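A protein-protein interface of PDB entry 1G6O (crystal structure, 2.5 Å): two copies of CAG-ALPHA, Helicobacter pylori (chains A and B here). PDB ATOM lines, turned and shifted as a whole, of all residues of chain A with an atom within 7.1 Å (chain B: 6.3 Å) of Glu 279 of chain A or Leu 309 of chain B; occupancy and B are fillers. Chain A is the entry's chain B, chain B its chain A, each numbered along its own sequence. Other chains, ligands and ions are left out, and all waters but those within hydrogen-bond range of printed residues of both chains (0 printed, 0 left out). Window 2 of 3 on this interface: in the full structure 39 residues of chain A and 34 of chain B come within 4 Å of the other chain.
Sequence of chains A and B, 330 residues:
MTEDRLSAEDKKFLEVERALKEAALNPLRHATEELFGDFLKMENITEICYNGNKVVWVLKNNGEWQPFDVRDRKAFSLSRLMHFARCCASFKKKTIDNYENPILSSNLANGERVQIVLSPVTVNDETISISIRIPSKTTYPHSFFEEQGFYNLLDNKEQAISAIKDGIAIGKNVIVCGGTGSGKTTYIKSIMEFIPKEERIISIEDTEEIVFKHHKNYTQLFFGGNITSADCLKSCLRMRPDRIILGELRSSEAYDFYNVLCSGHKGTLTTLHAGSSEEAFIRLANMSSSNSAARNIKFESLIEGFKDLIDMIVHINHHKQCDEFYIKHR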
ATOM      1  N   CYS A 177      -1.873 -24.688  -5.661  1.00  0.00           N
ATOM      2  CA  CYS A 177      -0.841 -24.400  -4.688  1.00  0.00           C
ATOM      3  C   CYS A 177      -0.561 -22.916  -4.558  1.00  0.00           C
ATOM      4  O   CYS A 177      -1.034 -22.098  -5.343  1.00  0.00           O
ATOM      5  CB  CYS A 177       0.449 -25.153  -5.041  1.00  0.00           C
ATOM      6  SG  CYS A 177       1.216 -24.693  -6.604  1.00  0.00           S
ATOM      7  N   LEU A 272      -1.939 -27.632  -2.010  1.00  0.00           N
ATOM      8  CA  LEU A 272      -0.575 -27.810  -1.515  1.00  0.00           C
ATOM      9  C   LEU A 272       0.195 -26.492  -1.324  1.00  0.00           C
ATOM     10  O   LEU A 272      -0.024 -25.519  -2.048  1.00  0.00           O
ATOM     11  CB  LEU A 272       0.190 -28.676  -2.526  1.00  0.00           C
ATOM     12  CG  LEU A 272       1.688 -28.843  -2.311  1.00  0.00           C
ATOM     13  CD1 LEU A 272       1.962 -29.935  -1.321  1.00  0.00           C
ATOM     14  CD2 LEU A 272       2.356 -29.192  -3.601  1.00  0.00           C
ATOM     15  N   HIS A 273       1.101 -26.454  -0.356  1.00  0.00           N
ATOM     16  CA  HIS A 273       1.919 -25.257  -0.176  1.00  0.00           C
ATOM     17  C   HIS A 273       3.174 -25.397  -1.005  1.00  0.00           C
ATOM     18  O   HIS A 273       4.071 -26.149  -0.634  1.00  0.00           O
ATOM     19  CB  HIS A 273       2.364 -25.096   1.256  1.00  0.00           C
ATOM     20  CG  HIS A 273       1.384 -24.382   2.115  1.00  0.00           C
ATOM     21  ND1 HIS A 273       1.631 -24.113   3.443  1.00  0.00           N
ATOM     22  CD2 HIS A 273       0.155 -23.885   1.847  1.00  0.00           C
ATOM     23  CE1 HIS A 273       0.593 -23.481   3.957  1.00  0.00           C
ATOM     24  NE2 HIS A 273      -0.316 -23.330   3.010  1.00  0.00           N
ATOM     25  N   ALA A 274       3.240 -24.673  -2.116  1.00  0.00           N
ATOM     26  CA  ALA A 274       4.407 -24.708  -2.998  1.00  0.00           C
ATOM     27  C   ALA A 274       4.542 -23.364  -3.715  1.00  0.00           C
ATOM     28  O   ALA A 274       3.542 -22.707  -4.000  1.00  0.00           O
ATOM     29  CB  ALA A 274       4.265 -25.835  -4.006  1.00  0.00           C
ATOM     30  N   GLY A 275       5.775 -22.962  -4.014  1.00  0.00           N
ATOM     31  CA  GLY A 275       5.983 -21.686  -4.676  1.00  0.00           C
ATOM     32  C   GLY A 275       5.700 -21.652  -6.171  1.00  0.00           C
ATOM     33  O   GLY A 275       5.452 -20.588  -6.746  1.00  0.00           O
ATOM     34  N   SER A 276       5.718 -22.812  -6.809  1.00  0.00           N
ATOM     35  CA  SER A 276       5.506 -22.855  -8.240  1.00  0.00           C
ATOM     36  C   SER A 276       5.281 -24.272  -8.727  1.00  0.00           C
ATOM     37  O   SER A 276       5.421 -25.227  -7.964  1.00  0.00           O
ATOM     38  CB  SER A 276       6.731 -22.260  -8.949  1.00  0.00           C
ATOM     39  OG  SER A 276       7.936 -22.921  -8.574  1.00  0.00           O
ATOM     40  N   SER A 277       4.936 -24.397 -10.004  1.00  0.00           N
ATOM     41  CA  SER A 277       4.701 -25.698 -10.613  1.00  0.00           C
ATOM     42  C   SER A 277       5.843 -26.645 -10.289  1.00  0.00           C
ATOM     43  O   SER A 277       5.648 -27.650  -9.605  1.00  0.00           O
ATOM     44  CB  SER A 277       4.582 -25.573 -12.134  1.00  0.00           C
ATOM     45  OG  SER A 277       4.332 -26.836 -12.732  1.00  0.00           O
ATOM     46  N   GLU A 278       7.033 -26.315 -10.787  1.00  0.00           N
ATOM     47  CA  GLU A 278       8.222 -27.140 -10.564  1.00  0.00           C
ATOM     48  C   GLU A 278       8.518 -27.401  -9.084  1.00  0.00           C
ATOM     49  O   GLU A 278       8.933 -28.501  -8.718  1.00  0.00           O
ATOM     50  CB  GLU A 278       9.449 -26.506 -11.234  1.00  0.00           C
ATOM     51  CG  GLU A 278      10.594 -27.497 -11.457  1.00  0.00           C
ATOM     52  CD  GLU A 278      10.138 -28.781 -12.165  1.00  0.00           C
ATOM     53  OE1 GLU A 278       9.571 -28.694 -13.281  1.00  0.00           O
ATOM     54  OE2 GLU A 278      10.351 -29.882 -11.602  1.00  0.00           O
ATOM     55  N   GLU A 279       8.324 -26.394  -8.238  1.00  0.00           N
ATOM     56  CA  GLU A 279       8.557 -26.570  -6.800  1.00  0.00           C
ATOM     57  C   GLU A 279       7.553 -27.569  -6.212  1.00  0.00           C
ATOM     58  O   GLU A 279       7.825 -28.234  -5.202  1.00  0.00           O
ATOM     59  CB  GLU A 279       8.460 -25.228  -6.059  1.00  0.00           C
ATOM     60  CG  GLU A 279       9.710 -24.362  -6.221  1.00  0.00           C
ATOM     61  CD  GLU A 279       9.611 -23.025  -5.517  1.00  0.00           C
ATOM     62  OE1 GLU A 279       9.483 -22.997  -4.268  1.00  0.00           O
ATOM     63  OE2 GLU A 279       9.665 -21.995  -6.230  1.00  0.00           O
ATOM     64  N   ALA A 280       6.398 -27.670  -6.866  1.00  0.00           N
ATOM     65  CA  ALA A 280       5.344 -28.585  -6.451  1.00  0.00           C
ATOM     66  C   ALA A 280       5.757 -30.026  -6.766  1.00  0.00           C
ATOM     67  O   ALA A 280       5.743 -30.877  -5.879  1.00  0.00           O
ATOM     68  CB  ALA A 280       4.036 -28.237  -7.160  1.00  0.00           C
ATOM     69  N   PHE A 281       6.127 -30.289  -8.021  1.00  0.00           N
ATOM     70  CA  PHE A 281       6.552 -31.627  -8.451  1.00  0.00           C
ATOM     71  C   PHE A 281       7.697 -32.167  -7.586  1.00  0.00           C
ATOM     72  O   PHE A 281       7.831 -33.383  -7.395  1.00  0.00           O
ATOM     73  CB  PHE A 281       7.009 -31.583  -9.908  1.00  0.00           C
ATOM     74  CG  PHE A 281       5.888 -31.476 -10.895  1.00  0.00           C
ATOM     75  CD1 PHE A 281       5.800 -30.382 -11.754  1.00  0.00           C
ATOM     76  CD2 PHE A 281       4.941 -32.494 -10.999  1.00  0.00           C
ATOM     77  CE1 PHE A 281       4.783 -30.305 -12.711  1.00  0.00           C
ATOM     78  CE2 PHE A 281       3.923 -32.427 -11.949  1.00  0.00           C
ATOM     79  CZ  PHE A 281       3.843 -31.332 -12.808  1.00  0.00           C
ATOM     80  N   ILE A 282       8.523 -31.240  -7.090  1.00  0.00           N
ATOM     81  CA  ILE A 282       9.680 -31.549  -6.241  1.00  0.00           C
ATOM     82  C   ILE A 282       9.182 -31.774  -4.818  1.00  0.00           C
ATOM     83  O   ILE A 282       9.605 -32.713  -4.134  1.00  0.00           O
ATOM     84  CB  ILE A 282      10.735 -30.379  -6.239  1.00  0.00           C
ATOM     85  CG1 ILE A 282      11.161 -30.048  -7.677  1.00  0.00           C
ATOM     86  CG2 ILE A 282      11.967 -30.776  -5.410  1.00  0.00           C
ATOM     87  CD1 ILE A 282      12.186 -28.950  -7.787  1.00  0.00           C
ATOM     88  N   ARG A 283       8.275 -30.904  -4.385  1.00  0.00           N
ATOM     89  CA  ARG A 283       7.681 -30.990  -3.054  1.00  0.00           C
ATOM     90  C   ARG A 283       6.859 -32.292  -2.868  1.00  0.00           C
ATOM     91  O   ARG A 283       6.871 -32.872  -1.781  1.00  0.00           O
ATOM     92  CB  ARG A 283       6.801 -29.761  -2.815  1.00  0.00           C
ATOM     93  CG  ARG A 283       6.297 -29.640  -1.408  1.00  0.00           C
ATOM     94  CD  ARG A 283       7.424 -29.369  -0.445  1.00  0.00           C
ATOM     95  NE  ARG A 283       7.008 -29.549   0.946  1.00  0.00           N
ATOM     96  CZ  ARG A 283       6.009 -28.896   1.544  1.00  0.00           C
ATOM     97  NH1 ARG A 283       5.281 -27.994   0.889  1.00  0.00           N
ATOM     98  NH2 ARG A 283       5.742 -29.152   2.819  1.00  0.00           N
ATOM     99  N   LEU A 284       6.153 -32.745  -3.915  1.00  0.00           N
ATOM    100  CA  LEU A 284       5.361 -33.984  -3.847  1.00  0.00           C
ATOM    101  C   LEU A 284       6.275 -35.198  -3.693  1.00  0.00           C
ATOM    102  O   LEU A 284       5.912 -36.170  -3.033  1.00  0.00           O
ATOM    103  CB  LEU A 284       4.505 -34.168  -5.106  1.00  0.00           C
ATOM    104  CG  LEU A 284       3.284 -33.270  -5.274  1.00  0.00           C
ATOM    105  CD1 LEU A 284       2.638 -33.498  -6.623  1.00  0.00           C
ATOM    106  CD2 LEU A 284       2.309 -33.563  -4.165  1.00  0.00           C
ATOM    107  N   ALA A 285       7.449 -35.139  -4.323  1.00  0.00           N
ATOM    108  CA  ALA A 285       8.443 -36.216  -4.246  1.00  0.00           C
ATOM    109  C   ALA A 285       9.023 -36.267  -2.831  1.00  0.00           C
ATOM    110  O   ALA A 285       9.181 -37.340  -2.258  1.00  0.00           O
ATOM    111  CB  ALA A 285       9.552 -35.989  -5.264  1.00  0.00           C
ATOM    112  N   HIS A 315      -1.017 -22.084  -9.689  1.00  0.00           N
ATOM    113  CA  HIS A 315      -0.355 -21.406  -8.577  1.00  0.00           C
ATOM    114  C   HIS A 315      -0.988 -20.039  -8.360  1.00  0.00           C
ATOM    115  O   HIS A 315      -1.443 -19.411  -9.319  1.00  0.00           O
ATOM    116  CB  HIS A 315       1.148 -21.255  -8.852  1.00  0.00           C
ATOM    117  CG  HIS A 315       1.897 -20.509  -7.779  1.00  0.00           C
ATOM    118  ND1 HIS A 315       2.138 -19.149  -7.845  1.00  0.00           N
ATOM    119  CD2 HIS A 315       2.436 -20.930  -6.606  1.00  0.00           C
ATOM    120  CE1 HIS A 315       2.792 -18.770  -6.760  1.00  0.00           C
ATOM    121  NE2 HIS A 315       2.984 -19.830  -5.992  1.00  0.00           N
ATOM    122  N   GLU A 324       0.562 -18.492 -12.865  1.00  0.00           N
ATOM    123  CA  GLU A 324       1.121 -19.636 -13.583  1.00  0.00           C
ATOM    124  C   GLU A 324       0.052 -20.704 -13.753  1.00  0.00           C
ATOM    125  O   GLU A 324      -0.552 -21.140 -12.775  1.00  0.00           O
ATOM    126  CB  GLU A 324       2.346 -20.239 -12.871  1.00  0.00           C
ATOM    127  CG  GLU A 324       2.840 -21.521 -13.584  1.00  0.00           C
ATOM    128  CD  GLU A 324       4.048 -22.188 -12.930  1.00  0.00           C
ATOM    129  OE1 GLU A 324       4.283 -21.948 -11.723  1.00  0.00           O
ATOM    130  OE2 GLU A 324       4.753 -22.968 -13.617  1.00  0.00           O
ATOM    131  N   ASN B 173      15.289 -14.856   0.709  1.00  0.00           N
ATOM    132  CA  ASN B 173      15.913 -15.714   1.697  1.00  0.00           C
ATOM    133  C   ASN B 173      17.426 -15.451   1.796  1.00  0.00           C
ATOM    134  O   ASN B 173      18.216 -15.922   0.971  1.00  0.00           O
ATOM    135  CB  ASN B 173      15.636 -17.188   1.359  1.00  0.00           C
ATOM    136  CG  ASN B 173      14.137 -17.520   1.331  1.00  0.00           C
ATOM    137  OD1 ASN B 173      13.406 -17.280   2.300  1.00  0.00           O
ATOM    138  ND2 ASN B 173      13.682 -18.093   0.224  1.00  0.00           N
ATOM    139  N   TYR B 258      14.732 -26.595   5.262  1.00  0.00           N
ATOM    140  CA  TYR B 258      14.635 -26.892   3.828  1.00  0.00           C
ATOM    141  C   TYR B 258      13.206 -26.849   3.338  1.00  0.00           C
ATOM    142  O   TYR B 258      12.888 -26.134   2.393  1.00  0.00           O
ATOM    143  CB  TYR B 258      15.219 -28.284   3.529  1.00  0.00           C
ATOM    144  CG  TYR B 258      15.160 -28.716   2.069  1.00  0.00           C
ATOM    145  CD1 TYR B 258      15.621 -27.884   1.048  1.00  0.00           C
ATOM    146  CD2 TYR B 258      14.663 -29.975   1.715  1.00  0.00           C
ATOM    147  CE1 TYR B 258      15.586 -28.296  -0.290  1.00  0.00           C
ATOM    148  CE2 TYR B 258      14.624 -30.397   0.381  1.00  0.00           C
ATOM    149  CZ  TYR B 258      15.084 -29.558  -0.610  1.00  0.00           C
ATOM    150  OH  TYR B 258      15.035 -29.987  -1.919  1.00  0.00           O
ATOM    151  N   LEU B 261      11.539 -23.515   2.940  1.00  0.00           N
ATOM    152  CA  LEU B 261      11.882 -22.745   1.760  1.00  0.00           C
ATOM    153  C   LEU B 261      11.151 -23.348   0.557  1.00  0.00           C
ATOM    154  O   LEU B 261      10.680 -22.624  -0.329  1.00  0.00           O
ATOM    155  CB  LEU B 261      13.380 -22.785   1.463  1.00  0.00           C
ATOM    156  CG  LEU B 261      14.412 -21.926   2.247  1.00  0.00           C
ATOM    157  CD1 LEU B 261      14.017 -20.484   2.113  1.00  0.00           C
ATOM    158  CD2 LEU B 261      14.507 -22.405   3.676  1.00  0.00           C
ATOM    159  N   CYS B 262      11.033 -24.679   0.543  1.00  0.00           N
ATOM    160  CA  CYS B 262      10.344 -25.436  -0.523  1.00  0.00           C
ATOM    161  C   CYS B 262       8.822 -25.220  -0.657  1.00  0.00           C
ATOM    162  O   CYS B 262       8.243 -25.564  -1.683  1.00  0.00           O
ATOM    163  CB  CYS B 262      10.569 -26.931  -0.317  1.00  0.00           C
ATOM    164  SG  CYS B 262      12.231 -27.470  -0.618  1.00  0.00           S
ATOM    165  N   SER B 263       8.163 -24.740   0.392  1.00  0.00           N
ATOM    166  CA  SER B 263       6.720 -24.493   0.328  1.00  0.00           C
ATOM    167  C   SER B 263       6.603 -23.045  -0.179  1.00  0.00           C
ATOM    168  O   SER B 263       5.569 -22.386  -0.049  1.00  0.00           O
ATOM    169  CB  SER B 263       6.046 -24.629   1.704  1.00  0.00           C
ATOM    170  OG  SER B 263       6.480 -23.636   2.598  1.00  0.00           O
ATOM    171  N   GLY B 264       7.708 -22.568  -0.737  1.00  0.00           N
ATOM    172  CA  GLY B 264       7.751 -21.246  -1.294  1.00  0.00           C
ATOM    173  C   GLY B 264       7.470 -20.108  -0.326  1.00  0.00           C
ATOM    174  O   GLY B 264       6.970 -19.070  -0.746  1.00  0.00           O
ATOM    175  N   HIS B 265       7.843 -20.257   0.942  1.00  0.00           N
ATOM    176  CA  HIS B 265       7.616 -19.260   2.011  1.00  0.00           C
ATOM    177  C   HIS B 265       8.406 -17.907   1.992  1.00  0.00           C
ATOM    178  O   HIS B 265       9.580 -17.823   1.581  1.00  0.00           O
ATOM    179  CB  HIS B 265       7.816 -20.010   3.329  1.00  0.00           C
ATOM    180  CG  HIS B 265       7.421 -19.229   4.525  1.00  0.00           C
ATOM    181  ND1 HIS B 265       8.219 -18.231   5.050  1.00  0.00           N
ATOM    182  CD2 HIS B 265       6.327 -19.289   5.310  1.00  0.00           C
ATOM    183  CE1 HIS B 265       7.627 -17.716   6.109  1.00  0.00           C
ATOM    184  NE2 HIS B 265       6.480 -18.341   6.285  1.00  0.00           N
ATOM    185  N   GLU B 304      21.239 -28.994  -4.646  1.00  0.00           N
ATOM    186  CA  GLU B 304      20.609 -28.296  -5.748  1.00  0.00           C
ATOM    187  C   GLU B 304      19.340 -27.587  -5.291  1.00  0.00           C
ATOM    188  O   GLU B 304      18.898 -26.624  -5.915  1.00  0.00           O
ATOM    189  CB  GLU B 304      20.297 -29.265  -6.881  1.00  0.00           C
ATOM    190  CG  GLU B 304      21.500 -29.611  -7.744  1.00  0.00           C
ATOM    191  CD  GLU B 304      21.082 -29.975  -9.169  1.00  0.00           C
ATOM    192  OE1 GLU B 304      20.289 -29.203  -9.753  1.00  0.00           O
ATOM    193  OE2 GLU B 304      21.533 -31.014  -9.711  1.00  0.00           O
ATOM    194  N   GLY B 305      18.744 -28.068  -4.207  1.00  0.00           N
ATOM    195  CA  GLY B 305      17.558 -27.412  -3.696  1.00  0.00           C
ATOM    196  C   GLY B 305      17.905 -26.056  -3.091  1.00  0.00           C
ATOM    197  O   GLY B 305      17.389 -25.020  -3.543  1.00  0.00           O
ATOM    198  N   PHE B 306      18.794 -26.054  -2.096  1.00  0.00           N
ATOM    199  CA  PHE B 306      19.169 -24.826  -1.422  1.00  0.00           C
ATOM    200  C   PHE B 306      19.615 -23.798  -2.412  1.00  0.00           C
ATOM    201  O   PHE B 306      19.124 -22.671  -2.360  1.00  0.00           O
ATOM    202  CB  PHE B 306      20.239 -25.077  -0.347  1.00  0.00           C
ATOM    203  CG  PHE B 306      19.734 -25.870   0.839  1.00  0.00           C
ATOM    204  CD1 PHE B 306      19.921 -27.249   0.903  1.00  0.00           C
ATOM    205  CD2 PHE B 306      19.049 -25.236   1.886  1.00  0.00           C
ATOM    206  CE1 PHE B 306      19.444 -27.999   1.996  1.00  0.00           C
ATOM    207  CE2 PHE B 306      18.568 -25.974   2.986  1.00  0.00           C
ATOM    208  CZ  PHE B 306      18.765 -27.356   3.033  1.00  0.00           C
ATOM    209  N   LYS B 307      20.502 -24.198  -3.330  1.00  0.00           N
ATOM    210  CA  LYS B 307      21.000 -23.311  -4.400  1.00  0.00           C
ATOM    211  C   LYS B 307      19.884 -22.661  -5.242  1.00  0.00           C
ATOM    212  O   LYS B 307      20.111 -21.650  -5.897  1.00  0.00           O
ATOM    213  CB  LYS B 307      21.950 -24.055  -5.361  1.00  0.00           C
ATOM    214  CG  LYS B 307      23.341 -24.352  -4.857  1.00  0.00           C
ATOM    215  CD  LYS B 307      24.211 -24.853  -5.989  1.00  0.00           C
ATOM    216  CE  LYS B 307      25.605 -25.098  -5.489  1.00  0.00           C
ATOM    217  NZ  LYS B 307      26.525 -25.578  -6.519  1.00  0.00           N
ATOM    218  N   ASP B 308      18.692 -23.233  -5.228  1.00  0.00           N
ATOM    219  CA  ASP B 308      17.572 -22.711  -6.003  1.00  0.00           C
ATOM    220  C   ASP B 308      16.668 -21.850  -5.106  1.00  0.00           C
ATOM    221  O   ASP B 308      15.990 -20.921  -5.568  1.00  0.00           O
ATOM    222  CB  ASP B 308      16.798 -23.894  -6.538  1.00  0.00           C
ATOM    223  CG  ASP B 308      15.896 -23.534  -7.707  1.00  0.00           C
ATOM    224  OD1 ASP B 308      15.090 -22.603  -7.532  1.00  0.00           O
ATOM    225  OD2 ASP B 308      16.039 -24.204  -8.748  1.00  0.00           O
ATOM    226  N   LEU B 309      16.693 -22.133  -3.807  1.00  0.00           N
ATOM    227  CA  LEU B 309      15.874 -21.382  -2.847  1.00  0.00           C
ATOM    228  C   LEU B 309      16.587 -20.237  -2.132  1.00  0.00           C
ATOM    229  O   LEU B 309      15.938 -19.279  -1.714  1.00  0.00           O
ATOM    230  CB  LEU B 309      15.277 -22.341  -1.824  1.00  0.00           C
ATOM    231  CG  LEU B 309      14.398 -23.415  -2.489  1.00  0.00           C
ATOM    232  CD1 LEU B 309      14.164 -24.562  -1.505  1.00  0.00           C
ATOM    233  CD2 LEU B 309      13.131 -22.736  -2.990  1.00  0.00           C
ATOM    234  N   ILE B 310      17.910 -20.312  -1.984  1.00  0.00           N
ATOM    235  CA  ILE B 310      18.632 -19.216  -1.310  1.00  0.00           C
ATOM    236  C   ILE B 310      18.926 -18.068  -2.286  1.00  0.00           C
ATOM    237  O   ILE B 310      19.638 -18.230  -3.274  1.00  0.00           O
ATOM    238  CB  ILE B 310      19.963 -19.701  -0.655  1.00  0.00           C
ATOM    239  CG1 ILE B 310      19.685 -20.844   0.337  1.00  0.00           C
ATOM    240  CG2 ILE B 310      20.633 -18.549   0.081  1.00  0.00           C
ATOM    241  CD1 ILE B 310      18.759 -20.482   1.496  1.00  0.00           C
ATOM    242  N   ASP B 311      18.352 -16.908  -1.997  1.00  0.00           N
ATOM    243  CA  ASP B 311      18.497 -15.710  -2.822  1.00  0.00           C
ATOM    244  C   ASP B 311      19.828 -14.910  -2.685  1.00  0.00           C
ATOM    245  O   ASP B 311      20.218 -14.168  -3.601  1.00  0.00           O
ATOM    246  CB  ASP B 311      17.298 -14.794  -2.559  1.00  0.00           C
ATOM    247  CG  ASP B 311      15.956 -15.484  -2.849  1.00  0.00           C
ATOM    248  OD1 ASP B 311      15.709 -15.866  -4.013  1.00  0.00           O
ATOM    249  OD2 ASP B 311      15.136 -15.648  -1.922  1.00  0.00           O
ATOM    250  N   MET B 312      20.502 -15.014  -1.543  1.00  0.00           N
ATOM    251  CA  MET B 312      21.791 -14.338  -1.368  1.00  0.00           C
ATOM    252  C   MET B 312      22.483 -14.735  -0.082  1.00  0.00           C
ATOM    253  O   MET B 312      21.835 -14.922   0.932  1.00  0.00           O
ATOM    254  CB  MET B 312      21.688 -12.797  -1.487  1.00  0.00           C
ATOM    255  CG  MET B 312      20.677 -12.018  -0.646  1.00  0.00           C
ATOM    256  SD  MET B 312      20.689 -10.077  -1.137  1.00  0.00           S
ATOM    257  CE  MET B 312      19.234 -10.107  -2.386  1.00  0.00           C
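Of chain B, only Cys 262, Gly 264 and Leu 309 come within 4 Å of Glu 279 of chain A. Leu 309 of chain B touches just one residue of chain A: Glu 279 (3.9 Å). Of the printed residues of chain B, Arg 283 of chain A touches Cys 262 and Ser 263. Printed residues of chain A within 4 Å of Ser 263 of chain B: His 273, Ala 274, Gly 275 and Arg 283. Of the printed residues of chain A, Gly 264 of chain B touches Gly 275 and Glu 279. The nearest residue of chain B that does not touch Glu 279 of chain A is Leu 261 of chain B (4.1 Å). The nearest printed residue of chain A that does not touch Gly 264 of chain B is Ala 274 of chain A (4.4 Å).
Of the 17 printed residues of chain A, 5 touch a printed residue of chain B. Hydrophobic or aromatic side chains of chain B within 4 Å of the printed part of chain A: Leu 309.
No position is printed for both chains. Of the 9 pairs that touch across the chains among the printed residues, none has its exchanged pair printed and touching as well.
Among the printed residues, pairs that only touch across the chains: His 273 of chain A with Ser 263 of chain B (3.3 Å), Ala 274 of chain A with Ser 263 of chain B (3.9 Å), Gly 275 of chain A with Ser 263 of chain B (3.9 Å), Gly 275 of chain A with Gly 264 of chain B (3.8 Å), Glu 279 of chain A with Cys 262 of chain B (3.8 Å), Glu 279 of chain A with Gly 264 of chain B (3.9 Å), Glu 279 of chain A with Leu 309 of chain B (3.9 Å), Arg 283 of chain A with Cys 262 of chain B (3.98 Å) and Arg 283 of chain A with Ser 263 of chain B (3.5 Å).
The guanidinium group (NH1) of Arg 283 of chain A sits at hydrogen-bond distance from the backbone carbonyl oxygen (O) of His 273 of chain A, at 2.7 Å. The side-chain hydroxyl (OG) of Ser 276 of chain A sits at hydrogen-bond distance from the side-chain carboxylate (OE2) of Glu 279 of chain A, 3.1 Å away. ND2 of Asn 173 of chain B lies within hydrogen-bond range of O of Leu 309 of chain B, at 3.2 Å. NE2 of His 315 of chain A sits at hydrogen-bond distance from O of Gly 275 of chain A (2.7 Å). The backbone carbonyl oxygen (O) of Tyr 258 of chain B lies within hydrogen-bond range of the side-chain sulfur (SG) of Cys 262 of chain B.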
